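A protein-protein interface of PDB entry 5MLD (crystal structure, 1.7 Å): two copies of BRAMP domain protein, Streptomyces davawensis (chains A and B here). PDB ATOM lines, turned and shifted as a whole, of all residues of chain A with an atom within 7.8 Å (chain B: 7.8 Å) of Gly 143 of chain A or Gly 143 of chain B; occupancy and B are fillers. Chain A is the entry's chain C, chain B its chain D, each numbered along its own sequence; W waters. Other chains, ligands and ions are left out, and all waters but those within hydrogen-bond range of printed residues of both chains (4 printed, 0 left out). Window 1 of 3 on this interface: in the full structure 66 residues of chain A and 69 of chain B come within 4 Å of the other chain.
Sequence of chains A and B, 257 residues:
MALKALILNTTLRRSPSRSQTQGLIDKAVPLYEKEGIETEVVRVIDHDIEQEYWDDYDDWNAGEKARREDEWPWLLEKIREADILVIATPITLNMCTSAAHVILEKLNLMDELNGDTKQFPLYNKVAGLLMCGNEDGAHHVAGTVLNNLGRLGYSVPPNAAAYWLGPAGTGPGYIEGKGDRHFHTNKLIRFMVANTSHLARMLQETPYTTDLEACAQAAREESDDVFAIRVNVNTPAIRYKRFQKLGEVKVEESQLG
A ring nitrogen (ND1) of His 139 of chain B sits at hydrogen-bond distance from the side-chain amide oxygen of Asn 147 of chain A (3.5 Å).
His 139 of chain A touches Asn 147 of chain B.
CB of Ala 142 of chain A touches ND2 of Asn 147 of chain B (3.4 Å).
Gly 143 of chain A touches Gly 143 of chain B (O to CA, 3.4 Å).
Ala 142 of chain B touches Asn 147 of chain A (CB to ND2, 3.4 Å).
Of the printed residues of chain B, His 139 of chain A touches Asn 147.
Of chain B, only Gly 143 (3.4 Å) comes within 4 Å of Gly 143 of chain A.
Of the printed residues of chain B, Asn 147 of chain A touches His 139 (3.5 Å) and Ala 142 (3.4 Å).
Of the printed residues of chain A, His 139 of chain B touches Asn 147.
Ala 142 of chain B touches one residue of chain A.
Of chain A, only Gly 143 (3.4 Å) comes within 4 Å of Gly 143 of chain B.
Of the printed residues of chain A, Asn 147 of chain B touches His 139 (3.6 Å) and Ala 142 (3.4 Å).
The nearest residue of chain B that does not touch Gly 143 of chain A is Asn 147 of chain B (4.2 Å).
The nearest residue of chain A that does not touch Gly 143 of chain B is Asn 147 of chain A (4.1 Å).
The nearest printed residue of chain A that does not touch His 139 of chain B is Gly 143 of chain A (5.6 Å).
Hydrophobic or aromatic side chains of chain A that line the printed part of chain B: His 139 and Ala 142.
His 139 of chain A touches Asn 147 of chain B, and with the chains exchanged Asn 147 of chain A touches His 139 of chain B.
Ala 142 of chain A touches Asn 147 of chain B, and with the chains exchanged Asn 147 of chain A touches Ala 142 of chain B.
Gly 143 of chain B touches its own counterpart, Gly 143 of chain A.
Positions printed for both chains: 129, 131, 137, 138, 139, 140, 141, 142, 143, 144, 145, 146, 147, 148, 149 and 161.
Of the 5 pairs that touch across the chains among the printed residues, 5 have their exchanged pair printed and touching as well.
Water W4 bridges a ring nitrogen (ND1) of His 139 of chain A (2.7 Å) and the side-chain amide nitrogen of Asn 147 of chain B (2.8 Å).
Water W2 lies within hydrogen-bond range of a ring nitrogen (ND1) of His 139 of chain B (2.7 Å) and the side-chain amide nitrogen (ND2) of Asn 147 of chain A (2.9 Å).
Water W3 bridges the backbone carbonyl oxygen (O) of Gly 143 of chain B (3.1 Å) and the backbone carbonyl oxygen (O) of Gly 143 of chain A (3.3 Å).
Water W1 lies within hydrogen-bond range of the backbone carbonyl oxygen of His 140 of chain A and the side-chain hydroxyl of Thr 144 of chain B.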
ATOM      1  N   LEU A 129       6.945   2.937   9.522  1.00  0.00           N
ATOM      2  CA  LEU A 129       6.495   2.278   8.309  1.00  0.00           C
ATOM      3  C   LEU A 129       7.553   1.297   7.814  1.00  0.00           C
ATOM      4  O   LEU A 129       8.739   1.629   7.754  1.00  0.00           O
ATOM      5  CB  LEU A 129       6.173   3.336   7.243  1.00  0.00           C
ATOM      6  CG  LEU A 129       5.475   2.888   5.977  1.00  0.00           C
ATOM      7  CD1 LEU A 129       4.170   2.195   6.306  1.00  0.00           C
ATOM      8  CD2 LEU A 129       5.209   4.113   5.102  1.00  0.00           C
ATOM      9  N   MET A 131       8.085  -1.225   4.374  1.00  0.00           N
ATOM     10  CA  MET A 131       7.515  -1.510   3.069  1.00  0.00           C
ATOM     11  C   MET A 131       8.420  -2.460   2.306  1.00  0.00           C
ATOM     12  O   MET A 131       9.632  -2.496   2.517  1.00  0.00           O
ATOM     13  CB  MET A 131       7.304  -0.233   2.249  1.00  0.00           C
ATOM     14  CG  MET A 131       6.281   0.719   2.844  1.00  0.00           C
ATOM     15  SD  MET A 131       6.490   2.323   2.061  1.00  0.00           S
ATOM     16  CE  MET A 131       8.041   2.873   2.773  1.00  0.00           C
ATOM     17  N   GLY A 137       8.157   2.386  -5.432  1.00  0.00           N
ATOM     18  CA  GLY A 137       6.933   2.856  -4.817  1.00  0.00           C
ATOM     19  C   GLY A 137       7.057   3.243  -3.354  1.00  0.00           C
ATOM     20  O   GLY A 137       6.094   3.755  -2.772  1.00  0.00           O
ATOM     21  N   ALA A 138       8.239   3.041  -2.761  1.00  0.00           N
ATOM     22  CA  ALA A 138       8.384   3.184  -1.310  1.00  0.00           C
ATOM     23  C   ALA A 138       8.113   4.610  -0.834  1.00  0.00           C
ATOM     24  O   ALA A 138       7.353   4.818   0.118  1.00  0.00           O
ATOM     25  CB  ALA A 138       9.783   2.736  -0.874  1.00  0.00           C
ATOM     26  N   HIS A 139       8.742   5.614  -1.453  1.00  0.00           N
ATOM     27  CA  HIS A 139       8.547   6.964  -0.914  1.00  0.00           C
ATOM     28  C   HIS A 139       7.141   7.497  -1.206  1.00  0.00           C
ATOM     29  O   HIS A 139       6.577   8.247  -0.397  1.00  0.00           O
ATOM     30  CB  HIS A 139       9.644   7.900  -1.438  1.00  0.00           C
ATOM     31  CG  HIS A 139      11.020   7.508  -0.986  1.00  0.00           C
ATOM     32  ND1 HIS A 139      11.434   7.619   0.325  1.00  0.00           N
ATOM     33  CD2 HIS A 139      12.066   6.975  -1.662  1.00  0.00           C
ATOM     34  CE1 HIS A 139      12.679   7.189   0.431  1.00  0.00           C
ATOM     35  NE2 HIS A 139      13.083   6.785  -0.760  1.00  0.00           N
ATOM     36  N   HIS A 140       6.548   7.111  -2.333  1.00  0.00           N
ATOM     37  CA  HIS A 140       5.166   7.494  -2.618  1.00  0.00           C
ATOM     38  C   HIS A 140       4.207   6.905  -1.587  1.00  0.00           C
ATOM     39  O   HIS A 140       3.327   7.603  -1.067  1.00  0.00           O
ATOM     40  CB  HIS A 140       4.787   7.033  -4.019  1.00  0.00           C
ATOM     41  CG  HIS A 140       3.431   7.490  -4.452  1.00  0.00           C
ATOM     42  ND1 HIS A 140       2.744   6.901  -5.491  1.00  0.00           N
ATOM     43  CD2 HIS A 140       2.640   8.487  -3.989  1.00  0.00           C
ATOM     44  CE1 HIS A 140       1.583   7.511  -5.645  1.00  0.00           C
ATOM     45  NE2 HIS A 140       1.492   8.473  -4.744  1.00  0.00           N
ATOM     46  N   VAL A 141       4.363   5.610  -1.279  1.00  0.00           N
ATOM     47  CA  VAL A 141       3.508   4.970  -0.284  1.00  0.00           C
ATOM     48  C   VAL A 141       3.743   5.582   1.096  1.00  0.00           C
ATOM     49  O   VAL A 141       2.795   5.803   1.861  1.00  0.00           O
ATOM     50  CB  VAL A 141       3.753   3.445  -0.289  1.00  0.00           C
ATOM     51  CG1 VAL A 141       3.022   2.764   0.856  1.00  0.00           C
ATOM     52  CG2 VAL A 141       3.326   2.850  -1.622  1.00  0.00           C
ATOM     53  N   ALA A 142       5.003   5.886   1.434  1.00  0.00           N
ATOM     54  CA  ALA A 142       5.267   6.520   2.720  1.00  0.00           C
ATOM     55  C   ALA A 142       4.576   7.868   2.808  1.00  0.00           C
ATOM     56  O   ALA A 142       3.977   8.196   3.838  1.00  0.00           O
ATOM     57  CB  ALA A 142       6.771   6.681   2.962  1.00  0.00           C
ATOM     58  N   GLY A 143       4.649   8.660   1.735  1.00  0.00           N
ATOM     59  CA  GLY A 143       3.989   9.952   1.741  1.00  0.00           C
ATOM     60  C   GLY A 143       2.512   9.813   2.023  1.00  0.00           C
ATOM     61  O   GLY A 143       1.976  10.462   2.923  1.00  0.00           O
ATOM     62  N   THR A 144       1.860   8.889   1.320  1.00  0.00           N
ATOM     63  CA  THR A 144       0.415   8.748   1.426  1.00  0.00           C
ATOM     64  C   THR A 144       0.006   8.211   2.792  1.00  0.00           C
ATOM     65  O   THR A 144      -0.884   8.763   3.449  1.00  0.00           O
ATOM     66  CB  THR A 144      -0.092   7.827   0.319  1.00  0.00           C
ATOM     67  OG1 THR A 144       0.288   8.369  -0.955  1.00  0.00           O
ATOM     68  CG2 THR A 144      -1.595   7.688   0.396  1.00  0.00           C
ATOM     69  N   VAL A 145       0.634   7.126   3.234  1.00  0.00           N
ATOM     70  CA  VAL A 145       0.226   6.495   4.491  1.00  0.00           C
ATOM     71  C   VAL A 145       0.568   7.381   5.688  1.00  0.00           C
ATOM     72  O   VAL A 145      -0.269   7.593   6.577  1.00  0.00           O
ATOM     73  CB  VAL A 145       0.856   5.099   4.622  1.00  0.00           C
ATOM     74  CG1 VAL A 145       0.568   4.509   6.016  1.00  0.00           C
ATOM     75  CG2 VAL A 145       0.329   4.182   3.523  1.00  0.00           C
ATOM     76  N   LEU A 146       1.792   7.914   5.740  1.00  0.00           N
ATOM     77  CA  LEU A 146       2.173   8.693   6.919  1.00  0.00           C
ATOM     78  C   LEU A 146       1.443  10.031   6.966  1.00  0.00           C
ATOM     79  O   LEU A 146       1.250  10.598   8.051  1.00  0.00           O
ATOM     80  CB  LEU A 146       3.690   8.900   6.960  1.00  0.00           C
ATOM     81  CG  LEU A 146       4.521   7.641   7.259  1.00  0.00           C
ATOM     82  CD1 LEU A 146       6.007   7.907   7.062  1.00  0.00           C
ATOM     83  CD2 LEU A 146       4.260   7.120   8.678  1.00  0.00           C
ATOM     84  N   ASN A 147       1.033  10.559   5.812  1.00  0.00           N
ATOM     85  CA  ASN A 147       0.217  11.765   5.842  1.00  0.00           C
ATOM     86  C   ASN A 147      -1.155  11.455   6.423  1.00  0.00           C
ATOM     87  O   ASN A 147      -1.711  12.247   7.190  1.00  0.00           O
ATOM     88  CB  ASN A 147       0.096  12.366   4.439  1.00  0.00           C
ATOM     89  CG  ASN A 147      -0.872  13.538   4.391  1.00  0.00           C
ATOM     90  OD1 ASN A 147      -2.004  13.409   3.913  1.00  0.00           O
ATOM     91  ND2 ASN A 147      -0.444  14.676   4.912  1.00  0.00           N
ATOM     92  N   ASN A 148      -1.702  10.287   6.099  1.00  0.00           N
ATOM     93  CA  ASN A 148      -3.023   9.955   6.616  1.00  0.00           C
ATOM     94  C   ASN A 148      -2.983   9.717   8.120  1.00  0.00           C
ATOM     95  O   ASN A 148      -3.910  10.113   8.841  1.00  0.00           O
ATOM     96  CB  ASN A 148      -3.579   8.739   5.892  1.00  0.00           C
ATOM     97  CG  ASN A 148      -5.008   8.478   6.257  1.00  0.00           C
ATOM     98  OD1 ASN A 148      -5.929   9.044   5.662  1.00  0.00           O
ATOM     99  ND2 ASN A 148      -5.212   7.637   7.259  1.00  0.00           N
ATOM    100  N   LEU A 149      -1.917   9.077   8.613  1.00  0.00           N
ATOM    101  CA  LEU A 149      -1.809   8.791  10.041  1.00  0.00           C
ATOM    102  C   LEU A 149      -1.570  10.057  10.838  1.00  0.00           C
ATOM    103  O   LEU A 149      -2.037  10.182  11.981  1.00  0.00           O
ATOM    104  CB  LEU A 149      -0.680   7.794  10.288  1.00  0.00           C
ATOM    105  CG  LEU A 149      -0.915   6.384   9.718  1.00  0.00           C
ATOM    106  CD1 LEU A 149       0.304   5.488   9.923  1.00  0.00           C
ATOM    107  CD2 LEU A 149      -2.145   5.748  10.328  1.00  0.00           C
ATOM    108  N   ALA A 161      10.504   5.599   7.927  1.00  0.00           N
ATOM    109  CA  ALA A 161      10.044   4.635   6.933  1.00  0.00           C
ATOM    110  C   ALA A 161      11.242   3.852   6.429  1.00  0.00           C
ATOM    111  O   ALA A 161      12.194   4.442   5.910  1.00  0.00           O
ATOM    112  CB  ALA A 161       9.331   5.334   5.775  1.00  0.00           C
ATOM    113  N   LEU B 129       3.542  22.662   7.451  1.00  0.00           N
ATOM    114  CA  LEU B 129       3.243  22.927   6.059  1.00  0.00           C
ATOM    115  C   LEU B 129       2.005  23.804   5.967  1.00  0.00           C
ATOM    116  O   LEU B 129       1.028  23.589   6.688  1.00  0.00           O
ATOM    117  CB  LEU B 129       3.049  21.593   5.329  1.00  0.00           C
ATOM    118  CG  LEU B 129       3.107  21.530   3.818  1.00  0.00           C
ATOM    119  CD1 LEU B 129       4.468  21.971   3.310  1.00  0.00           C
ATOM    120  CD2 LEU B 129       2.862  20.095   3.429  1.00  0.00           C
ATOM    121  N   MET B 131      -0.347  25.193   2.679  1.00  0.00           N
ATOM    122  CA  MET B 131      -0.522  25.083   1.236  1.00  0.00           C
ATOM    123  C   MET B 131      -1.750  25.845   0.761  1.00  0.00           C
ATOM    124  O   MET B 131      -2.751  25.960   1.468  1.00  0.00           O
ATOM    125  CB  MET B 131      -0.640  23.624   0.793  1.00  0.00           C
ATOM    126  CG  MET B 131       0.602  22.802   1.026  1.00  0.00           C
ATOM    127  SD  MET B 131       0.182  21.054   1.006  1.00  0.00           S
ATOM    128  CE  MET B 131      -0.731  20.907   2.554  1.00  0.00           C
ATOM    129  N   GLY B 137      -4.902  19.057  -4.450  1.00  0.00           N
ATOM    130  CA  GLY B 137      -3.511  18.611  -4.383  1.00  0.00           C
ATOM    131  C   GLY B 137      -2.868  18.694  -3.011  1.00  0.00           C
ATOM    132  O   GLY B 137      -1.698  18.330  -2.842  1.00  0.00           O
ATOM    133  N   ALA B 138      -3.616  19.173  -2.019  1.00  0.00           N
ATOM    134  CA  ALA B 138      -3.020  19.463  -0.718  1.00  0.00           C
ATOM    135  C   ALA B 138      -2.434  18.211  -0.078  1.00  0.00           C
ATOM    136  O   ALA B 138      -1.288  18.212   0.384  1.00  0.00           O
ATOM    137  CB  ALA B 138      -4.062  20.095   0.200  1.00  0.00           C
ATOM    138  N   HIS B 139      -3.210  17.125  -0.019  1.00  0.00           N
ATOM    139  CA  HIS B 139      -2.704  15.956   0.691  1.00  0.00           C
ATOM    140  C   HIS B 139      -1.576  15.280  -0.076  1.00  0.00           C
ATOM    141  O   HIS B 139      -0.650  14.734   0.532  1.00  0.00           O
ATOM    142  CB  HIS B 139      -3.848  14.983   0.976  1.00  0.00           C
ATOM    143  CG  HIS B 139      -4.844  15.532   1.948  1.00  0.00           C
ATOM    144  ND1 HIS B 139      -4.566  15.678   3.288  1.00  0.00           N
ATOM    145  CD2 HIS B 139      -6.097  16.014   1.766  1.00  0.00           C
ATOM    146  CE1 HIS B 139      -5.613  16.211   3.895  1.00  0.00           C
ATOM    147  NE2 HIS B 139      -6.552  16.429   2.992  1.00  0.00           N
ATOM    148  N   HIS B 140      -1.624  15.326  -1.406  1.00  0.00           N
ATOM    149  CA  HIS B 140      -0.532  14.778  -2.196  1.00  0.00           C
ATOM    150  C   HIS B 140       0.762  15.543  -1.945  1.00  0.00           C
ATOM    151  O   HIS B 140       1.821  14.936  -1.728  1.00  0.00           O
ATOM    152  CB  HIS B 140      -0.908  14.813  -3.676  1.00  0.00           C
ATOM    153  CG  HIS B 140       0.080  14.127  -4.558  1.00  0.00           C
ATOM    154  ND1 HIS B 140       0.179  14.397  -5.906  1.00  0.00           N
ATOM    155  CD2 HIS B 140       1.021  13.191  -4.289  1.00  0.00           C
ATOM    156  CE1 HIS B 140       1.136  13.654  -6.431  1.00  0.00           C
ATOM    157  NE2 HIS B 140       1.663  12.916  -5.472  1.00  0.00           N
ATOM    158  N   VAL B 141       0.697  16.884  -1.984  1.00  0.00           N
ATOM    159  CA  VAL B 141       1.878  17.709  -1.709  1.00  0.00           C
ATOM    160  C   VAL B 141       2.369  17.473  -0.286  1.00  0.00           C
ATOM    161  O   VAL B 141       3.577  17.350  -0.034  1.00  0.00           O
ATOM    162  CB  VAL B 141       1.554  19.196  -1.959  1.00  0.00           C
ATOM    163  CG1 VAL B 141       2.722  20.118  -1.555  1.00  0.00           C
ATOM    164  CG2 VAL B 141       1.181  19.418  -3.429  1.00  0.00           C
ATOM    165  N   ALA B 142       1.442  17.408   0.671  1.00  0.00           N
ATOM    166  CA  ALA B 142       1.836  17.176   2.056  1.00  0.00           C
ATOM    167  C   ALA B 142       2.596  15.860   2.196  1.00  0.00           C
ATOM    168  O   ALA B 142       3.664  15.810   2.814  1.00  0.00           O
ATOM    169  CB  ALA B 142       0.602  17.208   2.964  1.00  0.00           C
ATOM    170  N   GLY B 143       2.093  14.797   1.577  1.00  0.00           N
ATOM    171  CA  GLY B 143       2.807  13.529   1.630  1.00  0.00           C
ATOM    172  C   GLY B 143       4.211  13.651   1.073  1.00  0.00           C
ATOM    173  O   GLY B 143       5.180  13.221   1.703  1.00  0.00           O
ATOM    174  N   THR B 144       4.342  14.265  -0.112  1.00  0.00           N
ATOM    175  CA  THR B 144       5.650  14.339  -0.763  1.00  0.00           C
ATOM    176  C   THR B 144       6.612  15.219   0.021  1.00  0.00           C
ATOM    177  O   THR B 144       7.775  14.853   0.229  1.00  0.00           O
ATOM    178  CB  THR B 144       5.500  14.864  -2.190  1.00  0.00           C
ATOM    179  OG1 THR B 144       4.583  14.030  -2.903  1.00  0.00           O
ATOM    180  CG2 THR B 144       6.871  14.899  -2.909  1.00  0.00           C
ATOM    181  N   VAL B 145       6.160  16.406   0.440  1.00  0.00           N
ATOM    182  CA  VAL B 145       7.095  17.342   1.054  1.00  0.00           C
ATOM    183  C   VAL B 145       7.485  16.879   2.459  1.00  0.00           C
ATOM    184  O   VAL B 145       8.671  16.888   2.827  1.00  0.00           O
ATOM    185  CB  VAL B 145       6.497  18.761   1.048  1.00  0.00           C
ATOM    186  CG1 VAL B 145       7.350  19.726   1.874  1.00  0.00           C
ATOM    187  CG2 VAL B 145       6.372  19.239  -0.394  1.00  0.00           C
ATOM    188  N   LEU B 146       6.508  16.446   3.256  1.00  0.00           N
ATOM    189  CA  LEU B 146       6.832  16.045   4.626  1.00  0.00           C
ATOM    190  C   LEU B 146       7.594  14.722   4.670  1.00  0.00           C
ATOM    191  O   LEU B 146       8.435  14.526   5.560  1.00  0.00           O
ATOM    192  CB  LEU B 146       5.551  15.995   5.471  1.00  0.00           C
ATOM    193  CG  LEU B 146       4.925  17.379   5.742  1.00  0.00           C
ATOM    194  CD1 LEU B 146       3.558  17.249   6.417  1.00  0.00           C
ATOM    195  CD2 LEU B 146       5.852  18.267   6.578  1.00  0.00           C
ATOM    196  N   ASN B 147       7.366  13.822   3.710  1.00  0.00           N
ATOM    197  CA  ASN B 147       8.201  12.627   3.654  1.00  0.00           C
ATOM    198  C   ASN B 147       9.652  13.003   3.396  1.00  0.00           C
ATOM    199  O   ASN B 147      10.565  12.449   4.016  1.00  0.00           O
ATOM    200  CB  ASN B 147       7.702  11.653   2.581  1.00  0.00           C
ATOM    201  CG  ASN B 147       8.653  10.466   2.377  1.00  0.00           C
ATOM    202  OD1 ASN B 147       9.406  10.413   1.401  1.00  0.00           O
ATOM    203  ND2 ASN B 147       8.629   9.532   3.307  1.00  0.00           N
ATOM    204  N   ASN B 148       9.882  13.973   2.506  1.00  0.00           N
ATOM    205  CA  ASN B 148      11.246  14.379   2.203  1.00  0.00           C
ATOM    206  C   ASN B 148      11.912  15.057   3.394  1.00  0.00           C
ATOM    207  O   ASN B 148      13.099  14.830   3.654  1.00  0.00           O
ATOM    208  CB  ASN B 148      11.268  15.315   1.004  1.00  0.00           C
ATOM    209  CG  ASN B 148      12.679  15.676   0.607  1.00  0.00           C
ATOM    210  OD1 ASN B 148      13.198  16.731   0.983  1.00  0.00           O
ATOM    211  ND2 ASN B 148      13.324  14.777  -0.126  1.00  0.00           N
ATOM    212  N   LEU B 149      11.183  15.925   4.101  1.00  0.00           N
ATOM    213  CA  LEU B 149      11.774  16.586   5.263  1.00  0.00           C
ATOM    214  C   LEU B 149      12.047  15.591   6.384  1.00  0.00           C
ATOM    215  O   LEU B 149      13.024  15.751   7.117  1.00  0.00           O
ATOM    216  CB  LEU B 149      10.869  17.722   5.749  1.00  0.00           C
ATOM    217  CG  LEU B 149      10.741  18.894   4.783  1.00  0.00           C
ATOM    218  CD1 LEU B 149       9.718  19.953   5.229  1.00  0.00           C
ATOM    219  CD2 LEU B 149      12.128  19.522   4.526  1.00  0.00           C
ATOM    220  N   ALA B 161      -0.177  19.904   8.575  1.00  0.00           N
ATOM    221  CA  ALA B 161      -0.375  20.474   7.246  1.00  0.00           C
ATOM    222  C   ALA B 161      -1.716  21.194   7.199  1.00  0.00           C
ATOM    223  O   ALA B 161      -2.770  20.569   7.366  1.00  0.00           O
ATOM    224  CB  ALA B 161      -0.314  19.395   6.166  1.00  0.00           C
HETATM  225  O   HOH W   1       3.752  10.960  -1.528  1.00  0.00           O
HETATM  226  O   HOH W   2      -2.465  16.710   4.605  1.00  0.00           O
HETATM  227  O   HOH W   3       4.226  12.278   4.536  1.00  0.00           O
HETATM  228  O   HOH W   4      10.390   7.405   2.757  1.00  0.00           O
